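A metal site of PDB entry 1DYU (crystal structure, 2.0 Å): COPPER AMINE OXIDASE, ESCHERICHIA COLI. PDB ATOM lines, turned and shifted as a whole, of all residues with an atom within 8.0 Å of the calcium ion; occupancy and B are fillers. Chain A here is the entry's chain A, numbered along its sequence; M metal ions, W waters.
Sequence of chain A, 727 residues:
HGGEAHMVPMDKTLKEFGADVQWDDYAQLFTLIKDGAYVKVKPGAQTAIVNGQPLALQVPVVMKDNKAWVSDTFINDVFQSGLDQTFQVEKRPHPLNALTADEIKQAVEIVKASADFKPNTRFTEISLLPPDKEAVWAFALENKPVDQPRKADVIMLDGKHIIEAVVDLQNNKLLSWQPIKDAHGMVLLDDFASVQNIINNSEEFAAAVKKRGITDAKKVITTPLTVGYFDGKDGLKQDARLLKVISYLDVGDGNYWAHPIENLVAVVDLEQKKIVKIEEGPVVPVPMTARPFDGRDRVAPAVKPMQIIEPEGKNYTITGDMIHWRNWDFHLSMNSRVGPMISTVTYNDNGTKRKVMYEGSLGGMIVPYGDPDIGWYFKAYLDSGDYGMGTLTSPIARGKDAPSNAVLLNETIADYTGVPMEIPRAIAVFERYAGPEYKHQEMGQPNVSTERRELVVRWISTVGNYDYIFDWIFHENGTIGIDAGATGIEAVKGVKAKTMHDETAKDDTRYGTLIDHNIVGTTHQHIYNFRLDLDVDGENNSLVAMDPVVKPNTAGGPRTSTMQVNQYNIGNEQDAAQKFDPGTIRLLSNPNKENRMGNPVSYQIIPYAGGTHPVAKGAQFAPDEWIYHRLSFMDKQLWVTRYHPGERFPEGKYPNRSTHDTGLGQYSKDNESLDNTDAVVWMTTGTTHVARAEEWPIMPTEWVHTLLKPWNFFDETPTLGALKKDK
The side-chain amino group (NZ) of Lys 133 is in salt-bridge range of the side-chain carboxylate (OD2) of Asp 535, 3.1 Å away. The backbone NH of Asp 535 sits at hydrogen-bond distance from the backbone carbonyl oxygen of Val 356 (3.1 Å). OD2 of Asp 535 is in hydrogen-bond range of NE1 of Trp 137, 2.8 Å away. NZ of Lys 133 lies within salt-bridge range of OD2 of Asp 678. The backbone carbonyl oxygen of Asp 678 sits at hydrogen-bond distance from the backbone NH of Tyr 643. The side-chain carboxylate (OD2) of Asp 533 is in salt-bridge range of the side-chain amino group (NZ) of Lys 133, 2.7 Å away. The backbone NH (N) of Tyr 358 lies within hydrogen-bond range of the backbone carbonyl oxygen (O) of Asp 533. The backbone NH (N) of Asp 533 is in hydrogen-bond range of the backbone carbonyl oxygen (O) of Glu 359 (2.7 Å).
Lys 133 touches the calcium ion.
OD1 of Asp 535 binds the calcium ion (2.3 Å). O of Leu 534 binds the calcium ion (2.3 Å). The calcium ion is bound by O of Ala 679 (2.4 Å). OD1 of Asp 678 is bound to the calcium ion (2.4 Å). OD1 of Asp 533 is bound to the calcium ion (2.4 Å). The calcium ion is bound by water W1 (2.5 Å). The calcium ion has six donor atoms within binding distance.
Water W1 lies within hydrogen-bond range of the backbone carbonyl oxygen of Glu 539 (2.7 Å), the side-chain amide nitrogen of Asn 541 (2.8 Å) and the backbone NH of Ala 679 (3.1 Å).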
ATOM      1  N   LYS A 133     -31.147 -21.457  10.783  1.00  0.00           N
ATOM      2  CA  LYS A 133     -29.771 -21.892  10.763  1.00  0.00           C
ATOM      3  C   LYS A 133     -29.501 -23.084   9.873  1.00  0.00           C
ATOM      4  O   LYS A 133     -28.520 -23.126   9.151  1.00  0.00           O
ATOM      5  CB  LYS A 133     -29.346 -22.089  12.225  1.00  0.00           C
ATOM      6  CG  LYS A 133     -28.010 -22.819  12.385  1.00  0.00           C
ATOM      7  CD  LYS A 133     -27.517 -22.668  13.827  1.00  0.00           C
ATOM      8  CE  LYS A 133     -26.214 -23.442  14.057  1.00  0.00           C
ATOM      9  NZ  LYS A 133     -25.701 -23.213  15.429  1.00  0.00           N
ATOM     10  N   TRP A 137     -26.996 -23.026   6.622  1.00  0.00           N
ATOM     11  CA  TRP A 137     -25.795 -23.845   6.481  1.00  0.00           C
ATOM     12  C   TRP A 137     -25.849 -24.668   5.209  1.00  0.00           C
ATOM     13  O   TRP A 137     -24.788 -24.887   4.620  1.00  0.00           O
ATOM     14  CB  TRP A 137     -25.531 -24.859   7.608  1.00  0.00           C
ATOM     15  CG  TRP A 137     -24.664 -24.434   8.748  1.00  0.00           C
ATOM     16  CD1 TRP A 137     -24.955 -24.442  10.078  1.00  0.00           C
ATOM     17  CD2 TRP A 137     -23.304 -23.974   8.651  1.00  0.00           C
ATOM     18  NE1 TRP A 137     -23.879 -24.031  10.823  1.00  0.00           N
ATOM     19  CE2 TRP A 137     -22.851 -23.717   9.949  1.00  0.00           C
ATOM     20  CE3 TRP A 137     -22.437 -23.747   7.576  1.00  0.00           C
ATOM     21  CZ2 TRP A 137     -21.572 -23.220  10.243  1.00  0.00           C
ATOM     22  CZ3 TRP A 137     -21.151 -23.268   7.823  1.00  0.00           C
ATOM     23  CH2 TRP A 137     -20.772 -23.031   9.149  1.00  0.00           C
ATOM     24  N   VAL A 356     -17.070 -24.346  11.427  1.00  0.00           N
ATOM     25  CA  VAL A 356     -16.294 -23.874  12.544  1.00  0.00           C
ATOM     26  C   VAL A 356     -17.201 -22.954  13.374  1.00  0.00           C
ATOM     27  O   VAL A 356     -17.302 -23.105  14.593  1.00  0.00           O
ATOM     28  CB  VAL A 356     -14.976 -23.128  12.190  1.00  0.00           C
ATOM     29  CG1 VAL A 356     -14.313 -22.506  13.409  1.00  0.00           C
ATOM     30  CG2 VAL A 356     -14.011 -24.050  11.484  1.00  0.00           C
ATOM     31  N   MET A 357     -17.818 -21.977  12.716  1.00  0.00           N
ATOM     32  CA  MET A 357     -18.689 -21.034  13.413  1.00  0.00           C
ATOM     33  C   MET A 357     -19.876 -20.581  12.572  1.00  0.00           C
ATOM     34  O   MET A 357     -19.706 -20.019  11.481  1.00  0.00           O
ATOM     35  CB  MET A 357     -17.852 -19.823  13.875  1.00  0.00           C
ATOM     36  CG  MET A 357     -18.634 -18.753  14.618  1.00  0.00           C
ATOM     37  SD  MET A 357     -17.666 -17.489  15.451  1.00  0.00           S
ATOM     38  CE  MET A 357     -17.073 -16.556  14.014  1.00  0.00           C
ATOM     39  N   TYR A 358     -21.098 -20.772  13.069  1.00  0.00           N
ATOM     40  CA  TYR A 358     -22.272 -20.327  12.298  1.00  0.00           C
ATOM     41  C   TYR A 358     -22.368 -18.795  12.355  1.00  0.00           C
ATOM     42  O   TYR A 358     -22.567 -18.198  11.310  1.00  0.00           O
ATOM     43  CB  TYR A 358     -23.563 -20.905  12.914  1.00  0.00           C
ATOM     44  CG  TYR A 358     -24.761 -20.412  12.130  1.00  0.00           C
ATOM     45  CD1 TYR A 358     -24.949 -20.788  10.803  1.00  0.00           C
ATOM     46  CD2 TYR A 358     -25.677 -19.565  12.721  1.00  0.00           C
ATOM     47  CE1 TYR A 358     -26.057 -20.314  10.093  1.00  0.00           C
ATOM     48  CE2 TYR A 358     -26.777 -19.068  12.030  1.00  0.00           C
ATOM     49  CZ  TYR A 358     -26.925 -19.449  10.714  1.00  0.00           C
ATOM     50  OH  TYR A 358     -28.007 -18.994  10.030  1.00  0.00           O
ATOM     51  N   GLU A 359     -22.233 -18.159  13.512  1.00  0.00           N
ATOM     52  CA  GLU A 359     -22.288 -16.689  13.585  1.00  0.00           C
ATOM     53  C   GLU A 359     -21.468 -16.264  14.805  1.00  0.00           C
ATOM     54  O   GLU A 359     -21.543 -16.913  15.868  1.00  0.00           O
ATOM     55  CB  GLU A 359     -23.673 -16.044  13.787  1.00  0.00           C
ATOM     56  CG  GLU A 359     -24.764 -16.442  12.819  1.00  0.00           C
ATOM     57  CD  GLU A 359     -26.104 -15.825  13.233  1.00  0.00           C
ATOM     58  OE1 GLU A 359     -26.853 -16.364  14.087  1.00  0.00           O
ATOM     59  OE2 GLU A 359     -26.433 -14.753  12.704  1.00  0.00           O
ATOM     60  N   ARG A 531     -20.380 -12.915  21.316  1.00  0.00           N
ATOM     61  CA  ARG A 531     -21.284 -14.051  21.184  1.00  0.00           C
ATOM     62  C   ARG A 531     -20.760 -14.850  19.992  1.00  0.00           C
ATOM     63  O   ARG A 531     -20.689 -14.367  18.828  1.00  0.00           O
ATOM     64  CB  ARG A 531     -22.713 -13.529  20.869  1.00  0.00           C
ATOM     65  CG  ARG A 531     -23.699 -14.678  20.620  1.00  0.00           C
ATOM     66  CD  ARG A 531     -25.095 -14.156  20.239  1.00  0.00           C
ATOM     67  NE  ARG A 531     -25.971 -15.278  19.953  1.00  0.00           N
ATOM     68  CZ  ARG A 531     -25.998 -15.979  18.835  1.00  0.00           C
ATOM     69  NH1 ARG A 531     -25.183 -15.712  17.818  1.00  0.00           N
ATOM     70  NH2 ARG A 531     -26.834 -17.009  18.691  1.00  0.00           N
ATOM     71  N   LEU A 532     -20.401 -16.110  20.274  1.00  0.00           N
ATOM     72  CA  LEU A 532     -19.850 -16.990  19.268  1.00  0.00           C
ATOM     73  C   LEU A 532     -20.539 -18.317  19.108  1.00  0.00           C
ATOM     74  O   LEU A 532     -20.285 -19.238  19.885  1.00  0.00           O
ATOM     75  CB  LEU A 532     -18.309 -17.204  19.511  1.00  0.00           C
ATOM     76  CG  LEU A 532     -17.545 -15.931  19.899  1.00  0.00           C
ATOM     77  CD1 LEU A 532     -16.256 -16.261  20.660  1.00  0.00           C
ATOM     78  CD2 LEU A 532     -17.206 -15.088  18.669  1.00  0.00           C
ATOM     79  N   ASP A 533     -21.407 -18.395  18.104  1.00  0.00           N
ATOM     80  CA  ASP A 533     -22.129 -19.607  17.821  1.00  0.00           C
ATOM     81  C   ASP A 533     -21.205 -20.551  17.037  1.00  0.00           C
ATOM     82  O   ASP A 533     -21.294 -20.757  15.833  1.00  0.00           O
ATOM     83  CB  ASP A 533     -23.394 -19.389  16.995  1.00  0.00           C
ATOM     84  CG  ASP A 533     -24.189 -20.625  16.699  1.00  0.00           C
ATOM     85  OD1 ASP A 533     -23.842 -21.669  17.299  1.00  0.00           O
ATOM     86  OD2 ASP A 533     -25.128 -20.642  15.887  1.00  0.00           O
ATOM     87  N   LEU A 534     -20.291 -21.166  17.783  1.00  0.00           N
ATOM     88  CA  LEU A 534     -19.334 -22.151  17.227  1.00  0.00           C
ATOM     89  C   LEU A 534     -20.124 -23.446  16.983  1.00  0.00           C
ATOM     90  O   LEU A 534     -20.907 -23.716  17.893  1.00  0.00           O
ATOM     91  CB  LEU A 534     -18.293 -22.522  18.337  1.00  0.00           C
ATOM     92  CG  LEU A 534     -17.357 -21.302  18.589  1.00  0.00           C
ATOM     93  CD1 LEU A 534     -16.310 -21.481  19.702  1.00  0.00           C
ATOM     94  CD2 LEU A 534     -16.630 -20.885  17.309  1.00  0.00           C
ATOM     95  N   ASP A 535     -19.921 -24.141  15.890  1.00  0.00           N
ATOM     96  CA  ASP A 535     -20.506 -25.413  15.479  1.00  0.00           C
ATOM     97  C   ASP A 535     -19.212 -26.150  15.074  1.00  0.00           C
ATOM     98  O   ASP A 535     -18.766 -26.102  13.917  1.00  0.00           O
ATOM     99  CB  ASP A 535     -21.390 -25.317  14.225  1.00  0.00           C
ATOM    100  CG  ASP A 535     -22.766 -24.715  14.494  1.00  0.00           C
ATOM    101  OD1 ASP A 535     -23.015 -24.432  15.674  1.00  0.00           O
ATOM    102  OD2 ASP A 535     -23.578 -24.487  13.561  1.00  0.00           O
ATOM    103  N   VAL A 536     -18.552 -26.827  16.025  1.00  0.00           N
ATOM    104  CA  VAL A 536     -17.311 -27.504  15.813  1.00  0.00           C
ATOM    105  C   VAL A 536     -17.444 -28.723  14.929  1.00  0.00           C
ATOM    106  O   VAL A 536     -17.775 -29.784  15.464  1.00  0.00           O
ATOM    107  CB  VAL A 536     -16.592 -27.782  17.119  1.00  0.00           C
ATOM    108  CG1 VAL A 536     -15.295 -28.530  16.898  1.00  0.00           C
ATOM    109  CG2 VAL A 536     -16.352 -26.532  17.937  1.00  0.00           C
ATOM    110  N   GLY A 538     -19.692 -29.418  13.226  1.00  0.00           N
ATOM    111  CA  GLY A 538     -21.066 -29.933  13.272  1.00  0.00           C
ATOM    112  C   GLY A 538     -21.833 -29.213  14.350  1.00  0.00           C
ATOM    113  O   GLY A 538     -21.160 -28.595  15.177  1.00  0.00           O
ATOM    114  N   GLU A 539     -23.160 -29.331  14.310  1.00  0.00           N
ATOM    115  CA  GLU A 539     -24.025 -28.705  15.316  1.00  0.00           C
ATOM    116  C   GLU A 539     -23.879 -29.172  16.743  1.00  0.00           C
ATOM    117  O   GLU A 539     -23.781 -28.433  17.730  1.00  0.00           O
ATOM    118  CB  GLU A 539     -25.499 -28.960  14.912  1.00  0.00           C
ATOM    119  CG  GLU A 539     -26.574 -28.356  15.802  1.00  0.00           C
ATOM    120  CD  GLU A 539     -27.982 -28.876  15.512  1.00  0.00           C
ATOM    121  OE1 GLU A 539     -28.147 -29.669  14.561  1.00  0.00           O
ATOM    122  OE2 GLU A 539     -28.989 -28.551  16.157  1.00  0.00           O
ATOM    123  N   ASN A 540     -23.920 -30.475  16.937  1.00  0.00           N
ATOM    124  CA  ASN A 540     -23.861 -31.134  18.241  1.00  0.00           C
ATOM    125  C   ASN A 540     -22.515 -31.222  18.925  1.00  0.00           C
ATOM    126  O   ASN A 540     -21.667 -32.017  18.513  1.00  0.00           O
ATOM    127  CB  ASN A 540     -24.492 -32.541  18.060  1.00  0.00           C
ATOM    128  CG  ASN A 540     -25.933 -32.402  17.544  1.00  0.00           C
ATOM    129  OD1 ASN A 540     -26.706 -31.611  18.042  1.00  0.00           O
ATOM    130  ND2 ASN A 540     -26.314 -33.130  16.493  1.00  0.00           N
ATOM    131  N   ASN A 541     -22.338 -30.414  19.955  1.00  0.00           N
ATOM    132  CA  ASN A 541     -21.069 -30.363  20.692  1.00  0.00           C
ATOM    133  C   ASN A 541     -21.262 -30.444  22.206  1.00  0.00           C
ATOM    134  O   ASN A 541     -22.368 -30.402  22.739  1.00  0.00           O
ATOM    135  CB  ASN A 541     -20.387 -29.006  20.372  1.00  0.00           C
ATOM    136  CG  ASN A 541     -20.111 -28.778  18.898  1.00  0.00           C
ATOM    137  OD1 ASN A 541     -20.016 -29.628  17.978  1.00  0.00           O
ATOM    138  ND2 ASN A 541     -19.977 -27.481  18.626  1.00  0.00           N
ATOM    139  N   LEU A 588     -14.608 -26.850  23.262  1.00  0.00           N
ATOM    140  CA  LEU A 588     -15.962 -27.010  22.730  1.00  0.00           C
ATOM    141  C   LEU A 588     -15.606 -28.190  21.810  1.00  0.00           C
ATOM    142  O   LEU A 588     -14.925 -28.015  20.812  1.00  0.00           O
ATOM    143  CB  LEU A 588     -16.616 -25.837  22.047  1.00  0.00           C
ATOM    144  CG  LEU A 588     -18.038 -26.184  21.577  1.00  0.00           C
ATOM    145  CD1 LEU A 588     -18.892 -26.444  22.819  1.00  0.00           C
ATOM    146  CD2 LEU A 588     -18.624 -25.007  20.780  1.00  0.00           C
ATOM    147  N   VAL A 640     -21.778 -20.602  28.233  1.00  0.00           N
ATOM    148  CA  VAL A 640     -22.125 -21.490  27.144  1.00  0.00           C
ATOM    149  C   VAL A 640     -23.638 -21.724  27.325  1.00  0.00           C
ATOM    150  O   VAL A 640     -24.096 -22.077  28.428  1.00  0.00           O
ATOM    151  CB  VAL A 640     -21.321 -22.783  27.023  1.00  0.00           C
ATOM    152  CG1 VAL A 640     -21.636 -23.479  25.713  1.00  0.00           C
ATOM    153  CG2 VAL A 640     -19.812 -22.560  27.158  1.00  0.00           C
ATOM    154  N   THR A 641     -24.419 -21.514  26.269  1.00  0.00           N
ATOM    155  CA  THR A 641     -25.872 -21.668  26.377  1.00  0.00           C
ATOM    156  C   THR A 641     -26.320 -22.429  25.153  1.00  0.00           C
ATOM    157  O   THR A 641     -25.548 -22.547  24.196  1.00  0.00           O
ATOM    158  CB  THR A 641     -26.605 -20.296  26.434  1.00  0.00           C
ATOM    159  OG1 THR A 641     -26.329 -19.552  25.222  1.00  0.00           O
ATOM    160  CG2 THR A 641     -26.100 -19.516  27.627  1.00  0.00           C
ATOM    161  N   ARG A 642     -27.535 -22.946  25.227  1.00  0.00           N
ATOM    162  CA  ARG A 642     -28.076 -23.683  24.120  1.00  0.00           C
ATOM    163  C   ARG A 642     -28.471 -22.665  23.047  1.00  0.00           C
ATOM    164  O   ARG A 642     -28.927 -21.579  23.393  1.00  0.00           O
ATOM    165  CB  ARG A 642     -29.304 -24.519  24.555  1.00  0.00           C
ATOM    166  CG  ARG A 642     -29.837 -25.178  23.296  1.00  0.00           C
ATOM    167  CD  ARG A 642     -29.059 -26.414  22.813  1.00  0.00           C
ATOM    168  NE  ARG A 642     -29.465 -27.579  23.604  1.00  0.00           N
ATOM    169  CZ  ARG A 642     -30.217 -27.862  24.669  1.00  0.00           C
ATOM    170  NH1 ARG A 642     -30.822 -26.910  25.341  1.00  0.00           N
ATOM    171  NH2 ARG A 642     -30.289 -29.125  25.066  1.00  0.00           N
ATOM    172  N   TYR A 643     -28.260 -23.022  21.782  1.00  0.00           N
ATOM    173  CA  TYR A 643     -28.604 -22.097  20.697  1.00  0.00           C
ATOM    174  C   TYR A 643     -30.126 -21.790  20.670  1.00  0.00           C
ATOM    175  O   TYR A 643     -30.906 -22.724  20.766  1.00  0.00           O
ATOM    176  CB  TYR A 643     -28.264 -22.756  19.372  1.00  0.00           C
ATOM    177  CG  TYR A 643     -28.775 -21.937  18.177  1.00  0.00           C
ATOM    178  CD1 TYR A 643     -28.213 -20.706  17.822  1.00  0.00           C
ATOM    179  CD2 TYR A 643     -29.864 -22.417  17.453  1.00  0.00           C
ATOM    180  CE1 TYR A 643     -28.740 -19.988  16.758  1.00  0.00           C
ATOM    181  CE2 TYR A 643     -30.395 -21.715  16.374  1.00  0.00           C
ATOM    182  CZ  TYR A 643     -29.806 -20.488  16.044  1.00  0.00           C
ATOM    183  OH  TYR A 643     -30.333 -19.813  14.985  1.00  0.00           O
ATOM    184  N   THR A 677     -25.104 -31.069  22.106  1.00  0.00           N
ATOM    185  CA  THR A 677     -26.229 -30.305  21.534  1.00  0.00           C
ATOM    186  C   THR A 677     -25.651 -29.005  20.938  1.00  0.00           C
ATOM    187  O   THR A 677     -24.446 -28.714  21.096  1.00  0.00           O
ATOM    188  CB  THR A 677     -27.204 -30.015  22.685  1.00  0.00           C
ATOM    189  OG1 THR A 677     -28.425 -29.487  22.180  1.00  0.00           O
ATOM    190  CG2 THR A 677     -26.641 -29.124  23.772  1.00  0.00           C
ATOM    191  N   ASP A 678     -26.480 -28.241  20.249  1.00  0.00           N
ATOM    192  CA  ASP A 678     -26.054 -26.953  19.619  1.00  0.00           C
ATOM    193  C   ASP A 678     -25.747 -25.937  20.714  1.00  0.00           C
ATOM    194  O   ASP A 678     -26.577 -25.401  21.456  1.00  0.00           O
ATOM    195  CB  ASP A 678     -27.096 -26.452  18.608  1.00  0.00           C
ATOM    196  CG  ASP A 678     -26.566 -25.308  17.730  1.00  0.00           C
ATOM    197  OD1 ASP A 678     -25.490 -24.735  17.962  1.00  0.00           O
ATOM    198  OD2 ASP A 678     -27.188 -24.911  16.742  1.00  0.00           O
ATOM    199  N   ALA A 679     -24.463 -25.587  20.886  1.00  0.00           N
ATOM    200  CA  ALA A 679     -24.044 -24.641  21.901  1.00  0.00           C
ATOM    201  C   ALA A 679     -23.599 -23.263  21.324  1.00  0.00           C
ATOM    202  O   ALA A 679     -23.234 -23.195  20.156  1.00  0.00           O
ATOM    203  CB  ALA A 679     -22.873 -25.202  22.721  1.00  0.00           C
ATOM    204  N   VAL A 680     -23.662 -22.237  22.148  1.00  0.00           N
ATOM    205  CA  VAL A 680     -23.279 -20.879  21.804  1.00  0.00           C
ATOM    206  C   VAL A 680     -22.321 -20.500  22.965  1.00  0.00           C
ATOM    207  O   VAL A 680     -22.656 -20.603  24.136  1.00  0.00           O
ATOM    208  CB  VAL A 680     -24.439 -19.867  21.663  1.00  0.00           C
ATOM    209  CG1 VAL A 680     -23.990 -18.447  21.364  1.00  0.00           C
ATOM    210  CG2 VAL A 680     -25.436 -20.165  20.542  1.00  0.00           C
ATOM    211  N   VAL A 681     -21.116 -20.061  22.612  1.00  0.00           N
ATOM    212  CA  VAL A 681     -20.121 -19.649  23.597  1.00  0.00           C
ATOM    213  C   VAL A 681     -20.112 -18.132  23.701  1.00  0.00           C
ATOM    214  O   VAL A 681     -20.157 -17.436  22.698  1.00  0.00           O
ATOM    215  CB  VAL A 681     -18.740 -20.055  23.011  1.00  0.00           C
ATOM    216  CG1 VAL A 681     -17.619 -19.325  23.744  1.00  0.00           C
ATOM    217  CG2 VAL A 681     -18.659 -21.602  23.094  1.00  0.00           C
HETATM  218 CA    CA M   1     -23.238 -23.929  17.914  1.00  0.00          CA
HETATM  219  O   HOH W   1     -22.511 -26.250  18.540  1.00  0.00           O
